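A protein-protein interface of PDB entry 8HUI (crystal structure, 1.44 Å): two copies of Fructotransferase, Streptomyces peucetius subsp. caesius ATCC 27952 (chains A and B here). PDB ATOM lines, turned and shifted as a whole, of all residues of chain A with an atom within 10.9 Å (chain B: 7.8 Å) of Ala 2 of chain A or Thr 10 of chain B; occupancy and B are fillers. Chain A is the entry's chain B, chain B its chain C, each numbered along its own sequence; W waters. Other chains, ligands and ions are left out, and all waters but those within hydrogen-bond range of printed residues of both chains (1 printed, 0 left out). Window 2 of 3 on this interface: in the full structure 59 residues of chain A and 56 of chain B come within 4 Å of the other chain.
The backbone NH of Ala 2 of chain A sits at hydrogen-bond distance from the side-chain hydroxyl of Thr 9 of chain B. OG1 of Thr 4 of chain A lies within hydrogen-bond range of O of Pro 52 of chain B (2.8 Å).
The backbone carbonyl oxygen of Thr 4 of chain A is in hydrogen-bond range of the backbone NH of Val 47 of chain A, at 2.9 Å. The backbone carbonyl oxygen of Val 47 of chain A lies within hydrogen-bond range of the backbone NH of Tyr 6 of chain A. O of Tyr 6 of chain B lies within hydrogen-bond range of N of Tyr 49 of chain B (2.8 Å). The side-chain hydroxyl (OG1) of Thr 9 of chain B is in hydrogen-bond range of the side-chain carboxylate (OD1) of Asp 7 of chain B (2.7 Å). N of Val 8 of chain B sits at hydrogen-bond distance from O of Tyr 49 of chain B (3.1 Å). The backbone carbonyl oxygen of Pro 51 of chain B sits at hydrogen-bond distance from the side-chain hydroxyl of Tyr 55 of chain B, at 2.7 Å.
Among the printed residues, pairs that only touch across the chains: Ala 2 of chain A with Thr 10 of chain B (3.9 Å), Ala 2 of chain A with Tyr 19 of chain B (3.8 Å), Ala 2 of chain A with Pro 51 of chain B (3.8 Å), Thr 4 of chain A with Pro 51 of chain B (3.8 Å), Val 5 of chain A with Pro 51 of chain B (3.7 Å), Pro 44 of chain A with Gly 53 of chain B (3.7 Å), Gly 45 of chain A with Pro 52 of chain B (3.7 Å), Ala 46 of chain A with Pro 52 of chain B (3.7 Å), Val 47 of chain A with Tyr 49 of chain B (3.8 Å) and Val 47 of chain A with Pro 52 of chain B (3.8 Å).
Of chain B, only Thr 9 (2.9 Å), Thr 10 (3.9 Å), Tyr 19 (3.8 Å) and Pro 51 (3.8 Å) come within 4 Å of Ala 2 of chain A. Asp 3 of chain A touches none of the printed residues of chain B. Ile 33 of chain A touches none of the printed residues of chain B. Printed residues of chain B within 4 Å of Gly 45 of chain A: Pro 52. Of chain A, only Ala 2 comes within 4 Å of Thr 9 of chain B. Thr 10 of chain B touches one residue of chain A. Of the printed residues of chain A, Tyr 19 of chain B touches Ala 2. Of chain A, only Ala 2, Thr 4 and Val 5 come within 4 Å of Pro 51 of chain B. The nearest residue of chain A that does not touch Thr 10 of chain B is Asp 3 of chain A (7.4 Å). The nearest printed residue of chain B that does not touch Val 47 of chain A is Pro 51 of chain B (5.9 Å).
Hydrophobic or aromatic side chains of chain B within 4 Å of the printed part of chain A: Tyr 19, Tyr 49, Pro 51 and Pro 52.
Positions printed for both chains: 5, 6, 7, 10 and 11.
Water W1 bridges the side-chain carboxylate (OD2) of Asp 7 of chain B and the backbone NH (N) of Ala 2 of chain A.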
ATOM      1  N   ALA A   2       7.298  -0.448  21.281  1.00  0.00           N
ATOM      2  CA  ALA A   2       7.590   0.348  20.087  1.00  0.00           C
ATOM      3  C   ALA A   2       6.391   1.195  19.708  1.00  0.00           C
ATOM      4  O   ALA A   2       5.244   0.823  19.993  1.00  0.00           O
ATOM      5  CB  ALA A   2       7.973  -0.551  18.916  1.00  0.00           C
ATOM      6  N   ASP A   3       6.647   2.312  19.026  1.00  0.00           N
ATOM      7  CA  ASP A   3       5.567   3.220  18.666  1.00  0.00           C
ATOM      8  C   ASP A   3       4.845   2.808  17.393  1.00  0.00           C
ATOM      9  O   ASP A   3       4.052   3.580  16.856  1.00  0.00           O
ATOM     10  CB  ASP A   3       6.050   4.676  18.560  1.00  0.00           C
ATOM     11  CG  ASP A   3       7.015   4.907  17.429  1.00  0.00           C
ATOM     12  OD1 ASP A   3       7.243   4.006  16.596  1.00  0.00           O
ATOM     13  OD2 ASP A   3       7.548   6.040  17.358  1.00  0.00           O
ATOM     14  N   THR A   4       5.096   1.601  16.911  1.00  0.00           N
ATOM     15  CA  THR A   4       4.432   1.074  15.730  1.00  0.00           C
ATOM     16  C   THR A   4       3.233   0.225  16.092  1.00  0.00           C
ATOM     17  O   THR A   4       2.650  -0.417  15.201  1.00  0.00           O
ATOM     18  CB  THR A   4       5.405   0.216  14.917  1.00  0.00           C
ATOM     19  OG1 THR A   4       5.956  -0.791  15.786  1.00  0.00           O
ATOM     20  CG2 THR A   4       6.524   1.066  14.294  1.00  0.00           C
ATOM     21  N   VAL A   5       2.862   0.187  17.368  1.00  0.00           N
ATOM     22  CA  VAL A   5       1.743  -0.603  17.863  1.00  0.00           C
ATOM     23  C   VAL A   5       0.707   0.357  18.415  1.00  0.00           C
ATOM     24  O   VAL A   5       0.998   1.131  19.336  1.00  0.00           O
ATOM     25  CB  VAL A   5       2.191  -1.580  18.958  1.00  0.00           C
ATOM     26  CG1 VAL A   5       1.009  -2.329  19.508  1.00  0.00           C
ATOM     27  CG2 VAL A   5       3.248  -2.549  18.408  1.00  0.00           C
ATOM     28  N   TYR A   6      -0.500   0.300  17.863  1.00  0.00           N
ATOM     29  CA  TYR A   6      -1.602   1.175  18.220  1.00  0.00           C
ATOM     30  C   TYR A   6      -2.810   0.336  18.611  1.00  0.00           C
ATOM     31  O   TYR A   6      -3.029  -0.750  18.068  1.00  0.00           O
ATOM     32  CB  TYR A   6      -2.038   2.029  17.020  1.00  0.00           C
ATOM     33  CG  TYR A   6      -1.005   2.967  16.430  1.00  0.00           C
ATOM     34  CD1 TYR A   6      -0.054   2.505  15.537  1.00  0.00           C
ATOM     35  CD2 TYR A   6      -1.001   4.323  16.755  1.00  0.00           C
ATOM     36  CE1 TYR A   6       0.875   3.342  14.968  1.00  0.00           C
ATOM     37  CE2 TYR A   6      -0.086   5.176  16.192  1.00  0.00           C
ATOM     38  CZ  TYR A   6       0.867   4.684  15.305  1.00  0.00           C
ATOM     39  OH  TYR A   6       1.805   5.528  14.735  1.00  0.00           O
ATOM     40  N   ASP A   7      -3.587   0.844  19.561  1.00  0.00           N
ATOM     41  CA  ASP A   7      -4.898   0.315  19.925  1.00  0.00           C
ATOM     42  C   ASP A   7      -5.877   1.466  19.756  1.00  0.00           C
ATOM     43  O   ASP A   7      -5.667   2.547  20.312  1.00  0.00           O
ATOM     44  CB  ASP A   7      -4.844  -0.167  21.377  1.00  0.00           C
ATOM     45  CG  ASP A   7      -6.170  -0.688  21.917  1.00  0.00           C
ATOM     46  OD1 ASP A   7      -7.231  -0.070  21.664  1.00  0.00           O
ATOM     47  OD2 ASP A   7      -6.131  -1.697  22.681  1.00  0.00           O
ATOM     48  N   THR A  10      -6.994   3.187  22.999  1.00  0.00           N
ATOM     49  CA  THR A  10      -6.055   3.744  23.967  1.00  0.00           C
ATOM     50  C   THR A  10      -5.063   4.726  23.370  1.00  0.00           C
ATOM     51  O   THR A  10      -4.364   5.402  24.132  1.00  0.00           O
ATOM     52  CB  THR A  10      -5.258   2.641  24.694  1.00  0.00           C
ATOM     53  OG1 THR A  10      -4.360   1.995  23.780  1.00  0.00           O
ATOM     54  CG2 THR A  10      -6.157   1.601  25.297  1.00  0.00           C
ATOM     55  N   TRP A  11      -4.973   4.833  22.046  1.00  0.00           N
ATOM     56  CA  TRP A  11      -4.004   5.733  21.442  1.00  0.00           C
ATOM     57  C   TRP A  11      -4.339   7.173  21.808  1.00  0.00           C
ATOM     58  O   TRP A  11      -5.449   7.644  21.559  1.00  0.00           O
ATOM     59  CB  TRP A  11      -4.004   5.558  19.925  1.00  0.00           C
ATOM     60  CG  TRP A  11      -3.023   6.473  19.250  1.00  0.00           C
ATOM     61  CD1 TRP A  11      -1.701   6.586  19.523  1.00  0.00           C
ATOM     62  CD2 TRP A  11      -3.289   7.387  18.176  1.00  0.00           C
ATOM     63  NE1 TRP A  11      -1.120   7.513  18.701  1.00  0.00           N
ATOM     64  CE2 TRP A  11      -2.076   8.026  17.866  1.00  0.00           C
ATOM     65  CE3 TRP A  11      -4.438   7.737  17.461  1.00  0.00           C
ATOM     66  CZ2 TRP A  11      -1.973   8.991  16.864  1.00  0.00           C
ATOM     67  CZ3 TRP A  11      -4.336   8.690  16.467  1.00  0.00           C
ATOM     68  CH2 TRP A  11      -3.111   9.307  16.177  1.00  0.00           C
ATOM     69  N   ILE A  29      -4.519   7.469  12.826  1.00  0.00           N
ATOM     70  CA  ILE A  29      -3.348   6.631  13.071  1.00  0.00           C
ATOM     71  C   ILE A  29      -2.471   6.556  11.829  1.00  0.00           C
ATOM     72  O   ILE A  29      -1.241   6.623  11.913  1.00  0.00           O
ATOM     73  CB  ILE A  29      -3.789   5.237  13.548  1.00  0.00           C
ATOM     74  CG1 ILE A  29      -4.402   5.328  14.949  1.00  0.00           C
ATOM     75  CG2 ILE A  29      -2.581   4.253  13.538  1.00  0.00           C
ATOM     76  CD1 ILE A  29      -5.093   4.041  15.416  1.00  0.00           C
ATOM     77  N   ASP A  32      -0.445   9.535  11.478  1.00  0.00           N
ATOM     78  CA  ASP A  32       0.655   9.487  12.434  1.00  0.00           C
ATOM     79  C   ASP A  32       1.775   8.593  11.931  1.00  0.00           C
ATOM     80  O   ASP A  32       2.951   8.960  11.992  1.00  0.00           O
ATOM     81  CB  ASP A  32       0.146   9.010  13.790  1.00  0.00           C
ATOM     82  CG  ASP A  32       1.209   9.098  14.874  1.00  0.00           C
ATOM     83  OD1 ASP A  32       1.678  10.230  15.141  1.00  0.00           O
ATOM     84  OD2 ASP A  32       1.580   8.059  15.463  1.00  0.00           O
ATOM     85  N   ILE A  33       1.427   7.407  11.423  1.00  0.00           N
ATOM     86  CA  ILE A  33       2.434   6.529  10.849  1.00  0.00           C
ATOM     87  C   ILE A  33       3.219   7.258   9.766  1.00  0.00           C
ATOM     88  O   ILE A  33       4.459   7.225   9.734  1.00  0.00           O
ATOM     89  CB  ILE A  33       1.758   5.260  10.299  1.00  0.00           C
ATOM     90  CG1 ILE A  33       1.242   4.383  11.441  1.00  0.00           C
ATOM     91  CG2 ILE A  33       2.705   4.478   9.428  1.00  0.00           C
ATOM     92  CD1 ILE A  33       0.188   3.384  10.993  1.00  0.00           C
ATOM     93  N   LYS A  36       5.854   9.620  11.007  1.00  0.00           N
ATOM     94  CA  LYS A  36       7.012   8.986  11.624  1.00  0.00           C
ATOM     95  C   LYS A  36       7.822   8.127  10.663  1.00  0.00           C
ATOM     96  O   LYS A  36       9.003   7.868  10.925  1.00  0.00           O
ATOM     97  CB  LYS A  36       6.566   8.090  12.791  1.00  0.00           C
ATOM     98  CG  LYS A  36       5.851   8.825  13.924  1.00  0.00           C
ATOM     99  CD  LYS A  36       5.665   7.912  15.128  1.00  0.00           C
ATOM    100  CE  LYS A  36       4.672   8.412  16.176  1.00  0.00           C
ATOM    101  NZ  LYS A  36       4.497   9.882  16.240  1.00  0.00           N
ATOM    102  N   GLN A  37       7.224   7.654   9.588  1.00  0.00           N
ATOM    103  CA  GLN A  37       7.864   6.722   8.660  1.00  0.00           C
ATOM    104  C   GLN A  37       7.943   7.411   7.303  1.00  0.00           C
ATOM    105  O   GLN A  37       7.008   7.347   6.506  1.00  0.00           O
ATOM    106  CB  GLN A  37       7.063   5.422   8.636  1.00  0.00           C
ATOM    107  CG  GLN A  37       7.050   4.706   9.992  1.00  0.00           C
ATOM    108  CD  GLN A  37       6.459   3.301   9.944  1.00  0.00           C
ATOM    109  OE1 GLN A  37       6.461   2.654   8.904  1.00  0.00           O
ATOM    110  NE2 GLN A  37       5.921   2.846  11.079  1.00  0.00           N
ATOM    111  N   PRO A  44       8.514   0.400   7.835  1.00  0.00           N
ATOM    112  CA  PRO A  44       8.187  -1.000   8.152  1.00  0.00           C
ATOM    113  C   PRO A  44       6.708  -1.240   8.368  1.00  0.00           C
ATOM    114  O   PRO A  44       6.279  -2.395   8.353  1.00  0.00           O
ATOM    115  CB  PRO A  44       9.005  -1.270   9.418  1.00  0.00           C
ATOM    116  CG  PRO A  44       9.120   0.083  10.061  1.00  0.00           C
ATOM    117  CD  PRO A  44       9.290   1.030   8.927  1.00  0.00           C
ATOM    118  N   GLY A  45       5.920  -0.200   8.582  1.00  0.00           N
ATOM    119  CA  GLY A  45       4.506  -0.367   8.822  1.00  0.00           C
ATOM    120  C   GLY A  45       4.152  -0.322  10.295  1.00  0.00           C
ATOM    121  O   GLY A  45       4.900   0.190  11.134  1.00  0.00           O
ATOM    122  N   ALA A  46       3.003  -0.922  10.624  1.00  0.00           N
ATOM    123  CA  ALA A  46       2.443  -0.777  11.956  1.00  0.00           C
ATOM    124  C   ALA A  46       1.375  -1.836  12.176  1.00  0.00           C
ATOM    125  O   ALA A  46       0.955  -2.516  11.237  1.00  0.00           O
ATOM    126  CB  ALA A  46       1.832   0.618  12.124  1.00  0.00           C
ATOM    127  N   VAL A  47       0.921  -1.952  13.424  1.00  0.00           N
ATOM    128  CA  VAL A  47      -0.238  -2.768  13.765  1.00  0.00           C
ATOM    129  C   VAL A  47      -1.253  -1.891  14.477  1.00  0.00           C
ATOM    130  O   VAL A  47      -0.897  -1.110  15.374  1.00  0.00           O
ATOM    131  CB  VAL A  47       0.130  -4.016  14.602  1.00  0.00           C
ATOM    132  CG1 VAL A  47       0.982  -3.661  15.755  1.00  0.00           C
ATOM    133  CG2 VAL A  47      -1.147  -4.735  15.097  1.00  0.00           C
ATOM    134  N   ILE A  48      -2.514  -2.026  14.071  1.00  0.00           N
ATOM    135  CA  ILE A  48      -3.665  -1.384  14.693  1.00  0.00           C
ATOM    136  C   ILE A  48      -4.538  -2.492  15.257  1.00  0.00           C
ATOM    137  O   ILE A  48      -5.086  -3.312  14.504  1.00  0.00           O
ATOM    138  CB  ILE A  48      -4.459  -0.528  13.698  1.00  0.00           C
ATOM    139  CG1 ILE A  48      -3.532   0.520  13.070  1.00  0.00           C
ATOM    140  CG2 ILE A  48      -5.636   0.127  14.424  1.00  0.00           C
ATOM    141  CD1 ILE A  48      -4.192   1.348  11.978  1.00  0.00           C
ATOM    142  N   VAL B   5       5.979 -13.025  29.286  1.00  0.00           N
ATOM    143  CA  VAL B   5       5.651 -12.239  28.104  1.00  0.00           C
ATOM    144  C   VAL B   5       6.719 -11.165  27.933  1.00  0.00           C
ATOM    145  O   VAL B   5       6.926 -10.342  28.832  1.00  0.00           O
ATOM    146  CB  VAL B   5       4.260 -11.609  28.242  1.00  0.00           C
ATOM    147  CG1 VAL B   5       3.963 -10.736  27.059  1.00  0.00           C
ATOM    148  CG2 VAL B   5       3.190 -12.686  28.428  1.00  0.00           C
ATOM    149  N   TYR B   6       7.374 -11.156  26.776  1.00  0.00           N
ATOM    150  CA  TYR B   6       8.427 -10.209  26.459  1.00  0.00           C
ATOM    151  C   TYR B   6       8.121  -9.525  25.138  1.00  0.00           C
ATOM    152  O   TYR B   6       7.508 -10.118  24.243  1.00  0.00           O
ATOM    153  CB  TYR B   6       9.761 -10.899  26.248  1.00  0.00           C
ATOM    154  CG  TYR B   6      10.296 -11.678  27.422  1.00  0.00           C
ATOM    155  CD1 TYR B   6       9.817 -12.939  27.724  1.00  0.00           C
ATOM    156  CD2 TYR B   6      11.312 -11.155  28.222  1.00  0.00           C
ATOM    157  CE1 TYR B   6      10.333 -13.671  28.792  1.00  0.00           C
ATOM    158  CE2 TYR B   6      11.839 -11.883  29.295  1.00  0.00           C
ATOM    159  CZ  TYR B   6      11.347 -13.134  29.569  1.00  0.00           C
ATOM    160  OH  TYR B   6      11.823 -13.898  30.619  1.00  0.00           O
ATOM    161  N   ASP B   7       8.590  -8.287  25.008  1.00  0.00           N
ATOM    162  CA  ASP B   7       8.565  -7.531  23.764  1.00  0.00           C
ATOM    163  C   ASP B   7       9.991  -7.047  23.571  1.00  0.00           C
ATOM    164  O   ASP B   7      10.545  -6.420  24.467  1.00  0.00           O
ATOM    165  CB  ASP B   7       7.563  -6.376  23.903  1.00  0.00           C
ATOM    166  CG  ASP B   7       7.541  -5.429  22.707  1.00  0.00           C
ATOM    167  OD1 ASP B   7       8.601  -5.085  22.162  1.00  0.00           O
ATOM    168  OD2 ASP B   7       6.432  -4.988  22.352  1.00  0.00           O
ATOM    169  N   VAL B   8      10.602  -7.365  22.429  1.00  0.00           N
ATOM    170  CA  VAL B   8      12.013  -7.062  22.226  1.00  0.00           C
ATOM    171  C   VAL B   8      12.322  -5.573  22.326  1.00  0.00           C
ATOM    172  O   VAL B   8      13.484  -5.199  22.567  1.00  0.00           O
ATOM    173  CB  VAL B   8      12.554  -7.618  20.893  1.00  0.00           C
ATOM    174  CG1 VAL B   8      12.360  -9.121  20.819  1.00  0.00           C
ATOM    175  CG2 VAL B   8      11.927  -6.933  19.672  1.00  0.00           C
ATOM    176  N   THR B   9      11.326  -4.720  22.122  1.00  0.00           N
ATOM    177  CA  THR B   9      11.523  -3.276  22.154  1.00  0.00           C
ATOM    178  C   THR B   9      11.215  -2.641  23.503  1.00  0.00           C
ATOM    179  O   THR B   9      11.560  -1.472  23.698  1.00  0.00           O
ATOM    180  CB  THR B   9      10.686  -2.561  21.076  1.00  0.00           C
ATOM    181  OG1 THR B   9       9.301  -2.572  21.422  1.00  0.00           O
ATOM    182  CG2 THR B   9      10.890  -3.188  19.715  1.00  0.00           C
ATOM    183  N   THR B  10      10.572  -3.351  24.431  1.00  0.00           N
ATOM    184  CA  THR B  10      10.259  -2.766  25.726  1.00  0.00           C
ATOM    185  C   THR B  10      10.930  -3.491  26.870  1.00  0.00           C
ATOM    186  O   THR B  10      10.873  -3.005  28.004  1.00  0.00           O
ATOM    187  CB  THR B  10       8.744  -2.712  25.968  1.00  0.00           C
ATOM    188  OG1 THR B  10       8.219  -4.038  26.125  1.00  0.00           O
ATOM    189  CG2 THR B  10       8.030  -2.006  24.832  1.00  0.00           C
ATOM    190  N   TRP B  11      11.561  -4.624  26.611  1.00  0.00           N
ATOM    191  CA  TRP B  11      12.215  -5.371  27.673  1.00  0.00           C
ATOM    192  C   TRP B  11      13.487  -4.633  28.065  1.00  0.00           C
ATOM    193  O   TRP B  11      14.403  -4.481  27.247  1.00  0.00           O
ATOM    194  CB  TRP B  11      12.546  -6.783  27.204  1.00  0.00           C
ATOM    195  CG  TRP B  11      13.105  -7.647  28.309  1.00  0.00           C
ATOM    196  CD1 TRP B  11      12.473  -8.029  29.460  1.00  0.00           C
ATOM    197  CD2 TRP B  11      14.409  -8.242  28.355  1.00  0.00           C
ATOM    198  NE1 TRP B  11      13.307  -8.817  30.218  1.00  0.00           N
ATOM    199  CE2 TRP B  11      14.497  -8.969  29.565  1.00  0.00           C
ATOM    200  CE3 TRP B  11      15.510  -8.242  27.488  1.00  0.00           C
ATOM    201  CZ2 TRP B  11      15.637  -9.678  29.930  1.00  0.00           C
ATOM    202  CZ3 TRP B  11      16.642  -8.952  27.854  1.00  0.00           C
ATOM    203  CH2 TRP B  11      16.695  -9.659  29.069  1.00  0.00           C
ATOM    204  N   ALA B  12      13.545  -4.173  29.317  1.00  0.00           N
ATOM    205  CA  ALA B  12      14.625  -3.301  29.774  1.00  0.00           C
ATOM    206  C   ALA B  12      15.911  -4.042  30.099  1.00  0.00           C
ATOM    207  O   ALA B  12      16.945  -3.393  30.263  1.00  0.00           O
ATOM    208  CB  ALA B  12      14.158  -2.502  30.994  1.00  0.00           C
ATOM    209  N   GLY B  13      15.892  -5.372  30.171  1.00  0.00           N
ATOM    210  CA  GLY B  13      17.081  -6.135  30.497  1.00  0.00           C
ATOM    211  C   GLY B  13      18.080  -6.274  29.380  1.00  0.00           C
ATOM    212  O   GLY B  13      19.158  -6.839  29.589  1.00  0.00           O
ATOM    213  N   ALA B  14      17.738  -5.781  28.189  1.00  0.00           N
ATOM    214  CA  ALA B  14      18.621  -5.872  27.035  1.00  0.00           C
ATOM    215  C   ALA B  14      19.786  -4.897  27.163  1.00  0.00           C
ATOM    216  O   ALA B  14      19.614  -3.748  27.579  1.00  0.00           O
ATOM    217  CB  ALA B  14      17.834  -5.531  25.770  1.00  0.00           C
ATOM    218  N   PRO B  18      17.504  -3.851  20.052  1.00  0.00           N
ATOM    219  CA  PRO B  18      17.046  -4.855  19.078  1.00  0.00           C
ATOM    220  C   PRO B  18      17.144  -4.395  17.644  1.00  0.00           C
ATOM    221  O   PRO B  18      17.200  -5.234  16.739  1.00  0.00           O
ATOM    222  CB  PRO B  18      15.582  -5.087  19.476  1.00  0.00           C
ATOM    223  CG  PRO B  18      15.181  -3.794  20.073  1.00  0.00           C
ATOM    224  CD  PRO B  18      16.380  -3.315  20.843  1.00  0.00           C
ATOM    225  N   TYR B  19      17.146  -3.090  17.390  1.00  0.00           N
ATOM    226  CA  TYR B  19      17.289  -2.606  16.025  1.00  0.00           C
ATOM    227  C   TYR B  19      18.696  -2.831  15.526  1.00  0.00           C
ATOM    228  O   TYR B  19      18.915  -3.016  14.311  1.00  0.00           O
ATOM    229  CB  TYR B  19      16.901  -1.120  15.946  1.00  0.00           C
ATOM    230  CG  TYR B  19      15.488  -0.887  16.406  1.00  0.00           C
ATOM    231  CD1 TYR B  19      14.412  -1.157  15.566  1.00  0.00           C
ATOM    232  CD2 TYR B  19      15.211  -0.456  17.696  1.00  0.00           C
ATOM    233  CE1 TYR B  19      13.114  -0.961  15.985  1.00  0.00           C
ATOM    234  CE2 TYR B  19      13.894  -0.282  18.123  1.00  0.00           C
ATOM    235  CZ  TYR B  19      12.859  -0.534  17.255  1.00  0.00           C
ATOM    236  OH  TYR B  19      11.559  -0.359  17.674  1.00  0.00           O
ATOM    237  N   VAL B  25      19.505  -9.602  21.582  1.00  0.00           N
ATOM    238  CA  VAL B  25      18.409  -9.345  22.511  1.00  0.00           C
ATOM    239  C   VAL B  25      17.645 -10.626  22.805  1.00  0.00           C
ATOM    240  O   VAL B  25      17.295 -10.904  23.955  1.00  0.00           O
ATOM    241  CB  VAL B  25      17.485  -8.234  21.983  1.00  0.00           C
ATOM    242  CG1 VAL B  25      16.258  -8.102  22.893  1.00  0.00           C
ATOM    243  CG2 VAL B  25      18.246  -6.911  21.864  1.00  0.00           C
ATOM    244  N   TYR B  49       7.410 -11.096  21.623  1.00  0.00           N
ATOM    245  CA  TYR B  49       6.747 -10.326  20.578  1.00  0.00           C
ATOM    246  C   TYR B  49       7.726  -9.366  19.919  1.00  0.00           C
ATOM    247  O   TYR B  49       8.537  -8.706  20.592  1.00  0.00           O
ATOM    248  CB  TYR B  49       5.584  -9.533  21.163  1.00  0.00           C
ATOM    249  CG  TYR B  49       4.806  -8.768  20.118  1.00  0.00           C
ATOM    250  CD1 TYR B  49       4.052  -9.435  19.164  1.00  0.00           C
ATOM    251  CD2 TYR B  49       4.833  -7.380  20.070  1.00  0.00           C
ATOM    252  CE1 TYR B  49       3.337  -8.756  18.192  1.00  0.00           C
ATOM    253  CE2 TYR B  49       4.107  -6.693  19.113  1.00  0.00           C
ATOM    254  CZ  TYR B  49       3.369  -7.391  18.173  1.00  0.00           C
ATOM    255  OH  TYR B  49       2.631  -6.723  17.192  1.00  0.00           O
ATOM    256  N   ILE B  50       7.679  -9.317  18.593  1.00  0.00           N
ATOM    257  CA  ILE B  50       8.466  -8.402  17.780  1.00  0.00           C
ATOM    258  C   ILE B  50       7.482  -7.440  17.126  1.00  0.00           C
ATOM    259  O   ILE B  50       6.762  -7.840  16.204  1.00  0.00           O
ATOM    260  CB  ILE B  50       9.245  -9.160  16.704  1.00  0.00           C
ATOM    261  CG1 ILE B  50      10.137 -10.246  17.324  1.00  0.00           C
ATOM    262  CG2 ILE B  50      10.066  -8.182  15.835  1.00  0.00           C
ATOM    263  CD1 ILE B  50      10.771 -11.153  16.296  1.00  0.00           C
ATOM    264  N   PRO B  51       7.439  -6.182  17.530  1.00  0.00           N
ATOM    265  CA  PRO B  51       6.554  -5.228  16.869  1.00  0.00           C
ATOM    266  C   PRO B  51       7.039  -4.919  15.466  1.00  0.00           C
ATOM    267  O   PRO B  51       8.194  -5.225  15.115  1.00  0.00           O
ATOM    268  CB  PRO B  51       6.634  -3.970  17.752  1.00  0.00           C
ATOM    269  CG  PRO B  51       7.430  -4.317  18.923  1.00  0.00           C
ATOM    270  CD  PRO B  51       8.135  -5.616  18.692  1.00  0.00           C
ATOM    271  N   PRO B  52       6.209  -4.282  14.642  1.00  0.00           N
ATOM    272  CA  PRO B  52       6.697  -3.823  13.341  1.00  0.00           C
ATOM    273  C   PRO B  52       7.936  -2.944  13.500  1.00  0.00           C
ATOM    274  O   PRO B  52       8.019  -2.110  14.408  1.00  0.00           O
ATOM    275  CB  PRO B  52       5.507  -3.048  12.768  1.00  0.00           C
ATOM    276  CG  PRO B  52       4.296  -3.640  13.472  1.00  0.00           C
ATOM    277  CD  PRO B  52       4.781  -3.967  14.849  1.00  0.00           C
ATOM    278  N   GLY B  53       8.897  -3.142  12.615  1.00  0.00           N
ATOM    279  CA  GLY B  53      10.171  -2.456  12.691  1.00  0.00           C
ATOM    280  C   GLY B  53      11.182  -3.140  11.810  1.00  0.00           C
ATOM    281  O   GLY B  53      10.984  -4.260  11.326  1.00  0.00           O
ATOM    282  N   TYR B  55      14.773  -4.589  12.020  1.00  0.00           N
ATOM    283  CA  TYR B  55      15.731  -5.054  13.008  1.00  0.00           C
ATOM    284  C   TYR B  55      16.876  -5.777  12.315  1.00  0.00           C
ATOM    285  O   TYR B  55      16.652  -6.724  11.558  1.00  0.00           O
ATOM    286  CB  TYR B  55      15.071  -6.030  13.971  1.00  0.00           C
ATOM    287  CG  TYR B  55      13.805  -5.529  14.613  1.00  0.00           C
ATOM    288  CD1 TYR B  55      12.578  -5.714  13.994  1.00  0.00           C
ATOM    289  CD2 TYR B  55      13.837  -4.860  15.834  1.00  0.00           C
ATOM    290  CE1 TYR B  55      11.428  -5.267  14.578  1.00  0.00           C
ATOM    291  CE2 TYR B  55      12.667  -4.413  16.429  1.00  0.00           C
ATOM    292  CZ  TYR B  55      11.474  -4.615  15.789  1.00  0.00           C
ATOM    293  OH  TYR B  55      10.340  -4.146  16.411  1.00  0.00           O
HETATM  294  O   HOH W   1       5.521  -2.607  21.205  1.00  0.00           O
